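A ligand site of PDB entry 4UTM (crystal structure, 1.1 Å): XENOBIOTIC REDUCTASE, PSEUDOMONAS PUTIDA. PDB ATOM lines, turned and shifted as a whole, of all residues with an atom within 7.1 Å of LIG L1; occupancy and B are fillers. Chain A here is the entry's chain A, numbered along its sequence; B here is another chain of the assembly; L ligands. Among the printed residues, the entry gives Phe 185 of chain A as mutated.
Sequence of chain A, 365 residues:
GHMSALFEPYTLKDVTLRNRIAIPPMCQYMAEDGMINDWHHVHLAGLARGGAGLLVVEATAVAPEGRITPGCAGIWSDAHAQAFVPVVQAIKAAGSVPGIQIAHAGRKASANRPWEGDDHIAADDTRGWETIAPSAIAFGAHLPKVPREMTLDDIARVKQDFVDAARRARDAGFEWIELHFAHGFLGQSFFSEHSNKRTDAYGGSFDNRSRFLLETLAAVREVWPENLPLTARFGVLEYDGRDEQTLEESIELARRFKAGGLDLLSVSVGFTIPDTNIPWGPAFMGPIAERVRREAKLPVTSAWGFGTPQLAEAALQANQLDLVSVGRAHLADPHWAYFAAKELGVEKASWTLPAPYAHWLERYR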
ATOM      1  N   PRO A  25     -16.831   0.417  26.432  1.00  0.00           N
ATOM      2  CA  PRO A  25     -16.944   1.645  27.223  1.00  0.00           C
ATOM      3  C   PRO A  25     -15.818   2.611  26.881  1.00  0.00           C
ATOM      4  O   PRO A  25     -14.655   2.245  26.842  1.00  0.00           O
ATOM      5  CB  PRO A  25     -16.853   1.138  28.664  1.00  0.00           C
ATOM      6  CG  PRO A  25     -16.166  -0.210  28.565  1.00  0.00           C
ATOM      7  CD  PRO A  25     -16.657  -0.783  27.285  1.00  0.00           C
ATOM      8  N   MET A  26     -16.190   3.873  26.649  1.00  0.00           N
ATOM      9  CA  MET A  26     -15.229   4.934  26.347  1.00  0.00           C
ATOM     10  C   MET A  26     -15.623   6.210  27.065  1.00  0.00           C
ATOM     11  O   MET A  26     -16.530   6.933  26.639  1.00  0.00           O
ATOM     12  CB  MET A  26     -15.082   5.208  24.844  1.00  0.00           C
ATOM     13  CG  MET A  26     -14.366   4.089  24.106  1.00  0.00           C
ATOM     14  SD  MET A  26     -14.169   4.444  22.339  1.00  0.00           S
ATOM     15  CE  MET A  26     -15.845   4.187  21.806  1.00  0.00           C
ATOM     16  N   CYS A  27     -14.957   6.482  28.159  1.00  0.00           N
ATOM     17  CA  CYS A  27     -15.077   7.724  28.904  1.00  0.00           C
ATOM     18  C   CYS A  27     -15.065   8.945  28.005  1.00  0.00           C
ATOM     19  O   CYS A  27     -14.213   9.068  27.115  1.00  0.00           O
ATOM     20  CB  CYS A  27     -13.935   7.864  29.933  1.00  0.00           C
ATOM     21  SG  CYS A  27     -14.148   6.849  31.408  1.00  0.00           S
ATOM     22  N   TYR A  29     -15.624  12.210  29.655  1.00  0.00           N
ATOM     23  CA  TYR A  29     -15.142  13.281  30.502  1.00  0.00           C
ATOM     24  C   TYR A  29     -15.994  14.552  30.408  1.00  0.00           C
ATOM     25  O   TYR A  29     -15.488  15.655  30.606  1.00  0.00           O
ATOM     26  CB  TYR A  29     -13.650  13.577  30.270  1.00  0.00           C
ATOM     27  CG  TYR A  29     -12.782  12.336  30.245  1.00  0.00           C
ATOM     28  CD1 TYR A  29     -12.248  11.817  31.419  1.00  0.00           C
ATOM     29  CD2 TYR A  29     -12.536  11.660  29.067  1.00  0.00           C
ATOM     30  CE1 TYR A  29     -11.461  10.673  31.412  1.00  0.00           C
ATOM     31  CE2 TYR A  29     -11.757  10.510  29.056  1.00  0.00           C
ATOM     32  CZ  TYR A  29     -11.228  10.024  30.223  1.00  0.00           C
ATOM     33  OH  TYR A  29     -10.442   8.882  30.153  1.00  0.00           O
ATOM     34  N   ALA A  59     -17.262   3.877  31.627  1.00  0.00           N
ATOM     35  CA  ALA A  59     -17.083   3.670  33.054  1.00  0.00           C
ATOM     36  C   ALA A  59     -17.880   4.696  33.845  1.00  0.00           C
ATOM     37  O   ALA A  59     -17.621   5.903  33.778  1.00  0.00           O
ATOM     38  CB  ALA A  59     -15.618   3.793  33.418  1.00  0.00           C
ATOM     39  N   ILE A  68     -12.891   8.525  37.770  1.00  0.00           N
ATOM     40  CA  ILE A  68     -11.506   8.801  37.406  1.00  0.00           C
ATOM     41  C   ILE A  68     -11.208  10.299  37.553  1.00  0.00           C
ATOM     42  O   ILE A  68     -10.184  10.681  38.107  1.00  0.00           O
ATOM     43  CB  ILE A  68     -11.161   8.303  35.996  1.00  0.00           C
ATOM     44  CG1 ILE A  68     -11.550   6.845  35.794  1.00  0.00           C
ATOM     45  CG2 ILE A  68      -9.665   8.496  35.743  1.00  0.00           C
ATOM     46  CD1 ILE A  68     -11.583   6.436  34.327  1.00  0.00           C
ATOM     47  N   GLN A 101     -20.949  -0.010  31.836  1.00  0.00           N
ATOM     48  CA  GLN A 101     -19.843  -0.437  32.671  1.00  0.00           C
ATOM     49  C   GLN A 101     -19.890   0.329  33.980  1.00  0.00           C
ATOM     50  O   GLN A 101     -19.817   1.561  33.952  1.00  0.00           O
ATOM     51  CB  GLN A 101     -18.507  -0.186  31.947  1.00  0.00           C
ATOM     52  CG  GLN A 101     -17.334  -0.745  32.721  1.00  0.00           C
ATOM     53  CD  GLN A 101     -16.024  -0.326  32.129  1.00  0.00           C
ATOM     54  OE1 GLN A 101     -15.752   0.865  32.038  1.00  0.00           O
ATOM     55  NE2 GLN A 101     -15.199  -1.282  31.699  1.00  0.00           N
ATOM     56  N   PRO A 114      -7.848  13.730  30.306  1.00  0.00           N
ATOM     57  CA  PRO A 114      -6.630  13.385  29.562  1.00  0.00           C
ATOM     58  C   PRO A 114      -6.030  14.548  28.770  1.00  0.00           C
ATOM     59  O   PRO A 114      -4.803  14.576  28.612  1.00  0.00           O
ATOM     60  CB  PRO A 114      -7.097  12.249  28.656  1.00  0.00           C
ATOM     61  CG  PRO A 114      -8.163  11.573  29.495  1.00  0.00           C
ATOM     62  CD  PRO A 114      -8.902  12.736  30.094  1.00  0.00           C
ATOM     63  N   ASP A 118      -3.892  14.816  32.446  1.00  0.00           N
ATOM     64  CA  ASP A 118      -3.960  13.359  32.579  1.00  0.00           C
ATOM     65  C   ASP A 118      -3.347  12.849  33.877  1.00  0.00           C
ATOM     66  O   ASP A 118      -3.168  11.660  34.025  1.00  0.00           O
ATOM     67  CB  ASP A 118      -3.301  12.671  31.364  1.00  0.00           C
ATOM     68  CG  ASP A 118      -3.787  11.245  31.167  1.00  0.00           C
ATOM     69  OD1 ASP A 118      -4.981  10.984  31.340  1.00  0.00           O
ATOM     70  OD2 ASP A 118      -2.948  10.374  30.815  1.00  0.00           O
ATOM     71  N   HIS A 180     -16.321  -3.266  36.102  1.00  0.00           N
ATOM     72  CA  HIS A 180     -14.992  -2.825  35.687  1.00  0.00           C
ATOM     73  C   HIS A 180     -13.923  -3.272  36.679  1.00  0.00           C
ATOM     74  O   HIS A 180     -13.576  -2.566  37.617  1.00  0.00           O
ATOM     75  CB  HIS A 180     -14.953  -1.311  35.556  1.00  0.00           C
ATOM     76  CG  HIS A 180     -13.780  -0.851  34.770  1.00  0.00           C
ATOM     77  ND1 HIS A 180     -12.748  -1.680  34.399  1.00  0.00           N
ATOM     78  CD2 HIS A 180     -13.533   0.360  34.198  1.00  0.00           C
ATOM     79  CE1 HIS A 180     -11.917  -1.001  33.634  1.00  0.00           C
ATOM     80  NE2 HIS A 180     -12.367   0.239  33.500  1.00  0.00           N
ATOM     81  N   ALA A 182     -10.849  -4.053  35.611  1.00  0.00           N
ATOM     82  CA  ALA A 182      -9.621  -3.960  34.824  1.00  0.00           C
ATOM     83  C   ALA A 182      -8.911  -2.621  35.008  1.00  0.00           C
ATOM     84  O   ALA A 182      -9.340  -1.756  35.760  1.00  0.00           O
ATOM     85  CB  ALA A 182      -9.926  -4.227  33.338  1.00  0.00           C
ATOM     86  N   HIS A 183      -7.770  -2.485  34.322  1.00  0.00           N
ATOM     87  CA  HIS A 183      -7.152  -1.180  34.059  1.00  0.00           C
ATOM     88  C   HIS A 183      -6.616  -0.491  35.295  1.00  0.00           C
ATOM     89  O   HIS A 183      -6.432   0.715  35.319  1.00  0.00           O
ATOM     90  CB  HIS A 183      -8.062  -0.282  33.203  1.00  0.00           C
ATOM     91  CG  HIS A 183      -8.430  -0.910  31.881  1.00  0.00           C
ATOM     92  ND1 HIS A 183      -9.402  -0.390  31.062  1.00  0.00           N
ATOM     93  CD2 HIS A 183      -7.956  -2.014  31.236  1.00  0.00           C
ATOM     94  CE1 HIS A 183      -9.515  -1.149  29.981  1.00  0.00           C
ATOM     95  NE2 HIS A 183      -8.632  -2.128  30.051  1.00  0.00           N
ATOM     96  N   PHE A 185      -7.783  -0.088  38.225  1.00  0.00           N
ATOM     97  CA  PHE A 185      -8.778   0.527  39.080  1.00  0.00           C
ATOM     98  C   PHE A 185      -9.053  -0.378  40.280  1.00  0.00           C
ATOM     99  O   PHE A 185      -8.260  -1.295  40.562  1.00  0.00           O
ATOM    100  CB  PHE A 185     -10.008   0.860  38.239  1.00  0.00           C
ATOM    101  CG  PHE A 185      -9.736   1.864  37.124  1.00  0.00           C
ATOM    102  CD1 PHE A 185      -9.070   3.050  37.370  1.00  0.00           C
ATOM    103  CD2 PHE A 185     -10.182   1.610  35.852  1.00  0.00           C
ATOM    104  CE1 PHE A 185      -8.898   3.972  36.345  1.00  0.00           C
ATOM    105  CE2 PHE A 185      -9.999   2.521  34.844  1.00  0.00           C
ATOM    106  CZ  PHE A 185      -9.356   3.700  35.070  1.00  0.00           C
ATOM    107  N   ARG A 233     -15.032  -6.770  32.884  1.00  0.00           N
ATOM    108  CA  ARG A 233     -13.769  -6.506  32.215  1.00  0.00           C
ATOM    109  C   ARG A 233     -12.674  -6.793  33.228  1.00  0.00           C
ATOM    110  O   ARG A 233     -12.752  -6.371  34.388  1.00  0.00           O
ATOM    111  CB  ARG A 233     -13.673  -5.085  31.684  1.00  0.00           C
ATOM    112  CG  ARG A 233     -12.569  -4.910  30.617  1.00  0.00           C
ATOM    113  CD  ARG A 233     -12.652  -3.618  29.844  1.00  0.00           C
ATOM    114  NE  ARG A 233     -12.116  -3.814  28.495  1.00  0.00           N
ATOM    115  CZ  ARG A 233     -12.073  -2.862  27.566  1.00  0.00           C
ATOM    116  NH1 ARG A 233     -12.403  -1.608  27.841  1.00  0.00           N
ATOM    117  NH2 ARG A 233     -11.703  -3.226  26.329  1.00  0.00           N
ATOM    118  N   SER A 268      -8.670  -7.913  29.012  1.00  0.00           N
ATOM    119  CA  SER A 268      -7.808  -6.764  28.824  1.00  0.00           C
ATOM    120  C   SER A 268      -6.456  -6.960  29.507  1.00  0.00           C
ATOM    121  O   SER A 268      -6.099  -8.065  29.905  1.00  0.00           O
ATOM    122  CB  SER A 268      -8.526  -5.489  29.295  1.00  0.00           C
ATOM    123  OG  SER A 268      -7.886  -4.363  28.732  1.00  0.00           O
ATOM    124  N   PHE A 271      -2.788  -2.826  33.521  1.00  0.00           N
ATOM    125  CA  PHE A 271      -2.379  -1.435  33.763  1.00  0.00           C
ATOM    126  C   PHE A 271      -2.284  -1.104  35.243  1.00  0.00           C
ATOM    127  O   PHE A 271      -2.576   0.016  35.686  1.00  0.00           O
ATOM    128  CB  PHE A 271      -3.287  -0.419  33.049  1.00  0.00           C
ATOM    129  CG  PHE A 271      -3.389  -0.594  31.560  1.00  0.00           C
ATOM    130  CD1 PHE A 271      -2.386  -0.144  30.724  1.00  0.00           C
ATOM    131  CD2 PHE A 271      -4.494  -1.196  30.988  1.00  0.00           C
ATOM    132  CE1 PHE A 271      -2.494  -0.277  29.345  1.00  0.00           C
ATOM    133  CE2 PHE A 271      -4.606  -1.350  29.615  1.00  0.00           C
ATOM    134  CZ  PHE A 271      -3.594  -0.895  28.802  1.00  0.00           C
ATOM    135  N   TRP A 280       2.061  -3.368  22.139  1.00  0.00           N
ATOM    136  CA  TRP A 280       0.980  -2.809  21.355  1.00  0.00           C
ATOM    137  C   TRP A 280       1.081  -3.204  19.883  1.00  0.00           C
ATOM    138  O   TRP A 280       2.150  -3.146  19.284  1.00  0.00           O
ATOM    139  CB  TRP A 280       1.016  -1.292  21.434  1.00  0.00           C
ATOM    140  CG  TRP A 280       0.986  -0.757  22.817  1.00  0.00           C
ATOM    141  CD1 TRP A 280       2.035  -0.214  23.514  1.00  0.00           C
ATOM    142  CD2 TRP A 280      -0.127  -0.714  23.686  1.00  0.00           C
ATOM    143  NE1 TRP A 280       1.631   0.158  24.772  1.00  0.00           N
ATOM    144  CE2 TRP A 280       0.306  -0.137  24.903  1.00  0.00           C
ATOM    145  CE3 TRP A 280      -1.462  -1.109  23.565  1.00  0.00           C
ATOM    146  CZ2 TRP A 280      -0.560   0.073  25.976  1.00  0.00           C
ATOM    147  CZ3 TRP A 280      -2.297  -0.920  24.635  1.00  0.00           C
ATOM    148  CH2 TRP A 280      -1.854  -0.334  25.828  1.00  0.00           C
ATOM    149  N   TRP A 304      -8.499  -3.389  20.930  1.00  0.00           N
ATOM    150  CA  TRP A 304      -7.241  -2.722  20.586  1.00  0.00           C
ATOM    151  C   TRP A 304      -6.831  -3.071  19.170  1.00  0.00           C
ATOM    152  O   TRP A 304      -6.215  -4.110  18.930  1.00  0.00           O
ATOM    153  CB  TRP A 304      -6.067  -2.953  21.548  1.00  0.00           C
ATOM    154  CG  TRP A 304      -4.918  -2.046  21.152  1.00  0.00           C
ATOM    155  CD1 TRP A 304      -4.040  -2.222  20.105  1.00  0.00           C
ATOM    156  CD2 TRP A 304      -4.567  -0.802  21.760  1.00  0.00           C
ATOM    157  NE1 TRP A 304      -3.155  -1.172  20.051  1.00  0.00           N
ATOM    158  CE2 TRP A 304      -3.464  -0.284  21.055  1.00  0.00           C
ATOM    159  CE3 TRP A 304      -5.077  -0.071  22.834  1.00  0.00           C
ATOM    160  CZ2 TRP A 304      -2.862   0.929  21.390  1.00  0.00           C
ATOM    161  CZ3 TRP A 304      -4.480   1.128  23.169  1.00  0.00           C
ATOM    162  CH2 TRP A 304      -3.373   1.614  22.454  1.00  0.00           C
ATOM    163  N   TRP B 360      -7.916  11.534  21.312  1.00  0.00           N
ATOM    164  CA  TRP B 360      -7.580  10.130  21.105  1.00  0.00           C
ATOM    165  C   TRP B 360      -7.214   9.791  19.681  1.00  0.00           C
ATOM    166  O   TRP B 360      -6.678   8.721  19.405  1.00  0.00           O
ATOM    167  CB  TRP B 360      -8.755   9.253  21.549  1.00  0.00           C
ATOM    168  CG  TRP B 360      -9.196   9.610  22.899  1.00  0.00           C
ATOM    169  CD1 TRP B 360     -10.286  10.344  23.227  1.00  0.00           C
ATOM    170  CD2 TRP B 360      -8.497   9.340  24.104  1.00  0.00           C
ATOM    171  NE1 TRP B 360     -10.318  10.541  24.581  1.00  0.00           N
ATOM    172  CE2 TRP B 360      -9.228   9.922  25.145  1.00  0.00           C
ATOM    173  CE3 TRP B 360      -7.309   8.660  24.403  1.00  0.00           C
ATOM    174  CZ2 TRP B 360      -8.847   9.822  26.452  1.00  0.00           C
ATOM    175  CZ3 TRP B 360      -6.918   8.578  25.696  1.00  0.00           C
ATOM    176  CH2 TRP B 360      -7.694   9.161  26.719  1.00  0.00           C
HETATM  177  C1  LIG L   1      -8.876   6.004  28.744  1.00  0.00           C
HETATM  178  C2  LIG L   1      -7.976   5.627  27.777  1.00  0.00           C
HETATM  179  C3  LIG L   1      -7.538   4.340  27.647  1.00  0.00           C
HETATM  180  C4  LIG L   1      -8.069   3.388  28.465  1.00  0.00           C
HETATM  181  C5  LIG L   1      -8.989   3.784  29.464  1.00  0.00           C
HETATM  182  C6  LIG L   1      -9.421   5.072  29.645  1.00  0.00           C
HETATM  183  C7  LIG L   1     -10.367   5.350  30.662  1.00  0.00           C
HETATM  184  C8  LIG L   1     -10.844   4.298  31.465  1.00  0.00           C
HETATM  185  C9  LIG L   1     -10.404   2.973  31.249  1.00  0.00           C
HETATM  186  O1  LIG L   1      -9.452   2.813  30.286  1.00  0.00           O
HETATM  187  O2  LIG L   1     -10.736   1.994  31.783  1.00  0.00           O
HETATM  188  O3  LIG L   1      -7.757   2.037  28.404  1.00  0.00           O
HETATM  189  C1  LG2 L   2     -11.226   3.977  26.646  1.00  0.00           C
HETATM  190  N1  LG2 L   2     -11.161   2.676  27.206  1.00  0.00           N
HETATM  191  C2  LG2 L   2     -11.985   2.399  28.341  1.00  0.00           C
HETATM  192  N2  LG2 L   2     -11.953   1.133  28.788  1.00  0.00           N
HETATM  193  C3  LG2 L   2     -12.794   0.811  29.851  1.00  0.00           C
HETATM  194  O1  LG2 L   2     -12.822  -0.348  30.273  1.00  0.00           O
HETATM  195  N3  LG2 L   2     -13.686   1.820  30.322  1.00  0.00           N
HETATM  196  C4  LG2 L   2     -13.727   3.089  29.865  1.00  0.00           C
HETATM  197  O2  LG2 L   2     -14.628   3.874  30.256  1.00  0.00           O
HETATM  198  C5  LG2 L   2     -12.704   3.416  28.943  1.00  0.00           C
HETATM  199  N4  LG2 L   2     -12.597   4.751  28.530  1.00  0.00           N
HETATM  200  C6  LG2 L   2     -11.908   4.976  27.296  1.00  0.00           C
HETATM  201  C7  LG2 L   2     -12.029   6.253  26.720  1.00  0.00           C
HETATM  202  C8  LG2 L   2     -11.529   6.490  25.420  1.00  0.00           C
HETATM  203  C9  LG2 L   2     -11.810   7.785  24.729  1.00  0.00           C
HETATM  204  C10 LG2 L   2     -10.762   5.457  24.784  1.00  0.00           C
HETATM  205  C11 LG2 L   2     -10.179   5.679  23.441  1.00  0.00           C
HETATM  206  C12 LG2 L   2     -10.585   4.237  25.405  1.00  0.00           C
HETATM  207  C13 LG2 L   2     -10.559   1.534  26.454  1.00  0.00           C
HETATM  208  C14 LG2 L   2     -11.429   1.131  25.260  1.00  0.00           C
HETATM  209  O3  LG2 L   2     -12.634   0.502  25.776  1.00  0.00           O
HETATM  210  C15 LG2 L   2     -10.740   0.157  24.282  1.00  0.00           C
HETATM  211  O4  LG2 L   2     -10.351  -1.008  25.051  1.00  0.00           O
HETATM  212  C16 LG2 L   2      -9.472   0.760  23.661  1.00  0.00           C
HETATM  213  O5  LG2 L   2      -9.787   2.074  23.124  1.00  0.00           O
HETATM  214  C17 LG2 L   2      -8.892  -0.147  22.566  1.00  0.00           C
HETATM  215  O6  LG2 L   2      -9.796  -0.327  21.498  1.00  0.00           O
HETATM  216  P1  LG2 L   2      -9.638   0.457  20.101  1.00  0.00           P
HETATM  217  O7  LG2 L   2      -9.813   1.933  20.409  1.00  0.00           O
HETATM  218  O8  LG2 L   2      -8.208   0.188  19.585  1.00  0.00           O
HETATM  219  O9  LG2 L   2     -10.723  -0.102  19.205  1.00  0.00           O
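N3 of LG2 L2 lies within hydrogen-bond range of OE1 of Gln 101, 2.9 Å away. NE2 of His 180 sits at hydrogen-bond distance from O1 of LG2 L2, 3.3 Å away. ND1 of His 183 is in hydrogen-bond range of O2 of LIG L1 (2.8 Å). N of Trp 304 is in hydrogen-bond range of O6 of LG2 L2 (3.4 Å). An oxygen (O1) of LG2 L2 is in hydrogen-bond range of the guanidinium group (NH1) of Arg 233, 2.8 Å away. O3 of LG2 L2 is in hydrogen-bond range of O of Pro 25 (2.9 Å). The backbone NH (N) of Ala 59 sits at hydrogen-bond distance from an oxygen (O2) of LG2 L2 (3.0 Å). N of Cys 27 lies close to O2 of LG2 L2, at 3.4 Å. An oxygen (O2) of LIG L1 sits at hydrogen-bond distance from a ring nitrogen (NE2) of His 180, at 2.9 Å. An oxygen (O2) of LG2 L2 lies within hydrogen-bond range of the side-chain sulfur (SG) of Cys 27 (3.2 Å).
Residues that only touch LIG L1: Tyr 29, Ile 68, Phe 185 and Trp 360 of chain B. Hydrophobic or aromatic side chains that line LIG L1: Ile 68, His 180, His 183, Phe 185 and Trp 360 of chain B. Along chain A the residues within 4 Å of LIG L1 span positions 29 to 185.
N3 of LG2 L2 sits close to O2 of LIG L1 (3.3 Å).
ND1 of His 180 sits at hydrogen-bond distance from N of Ala 182, 3.3 Å away. NE2 of His 183 sits at hydrogen-bond distance from OG of Ser 268 (2.7 Å).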
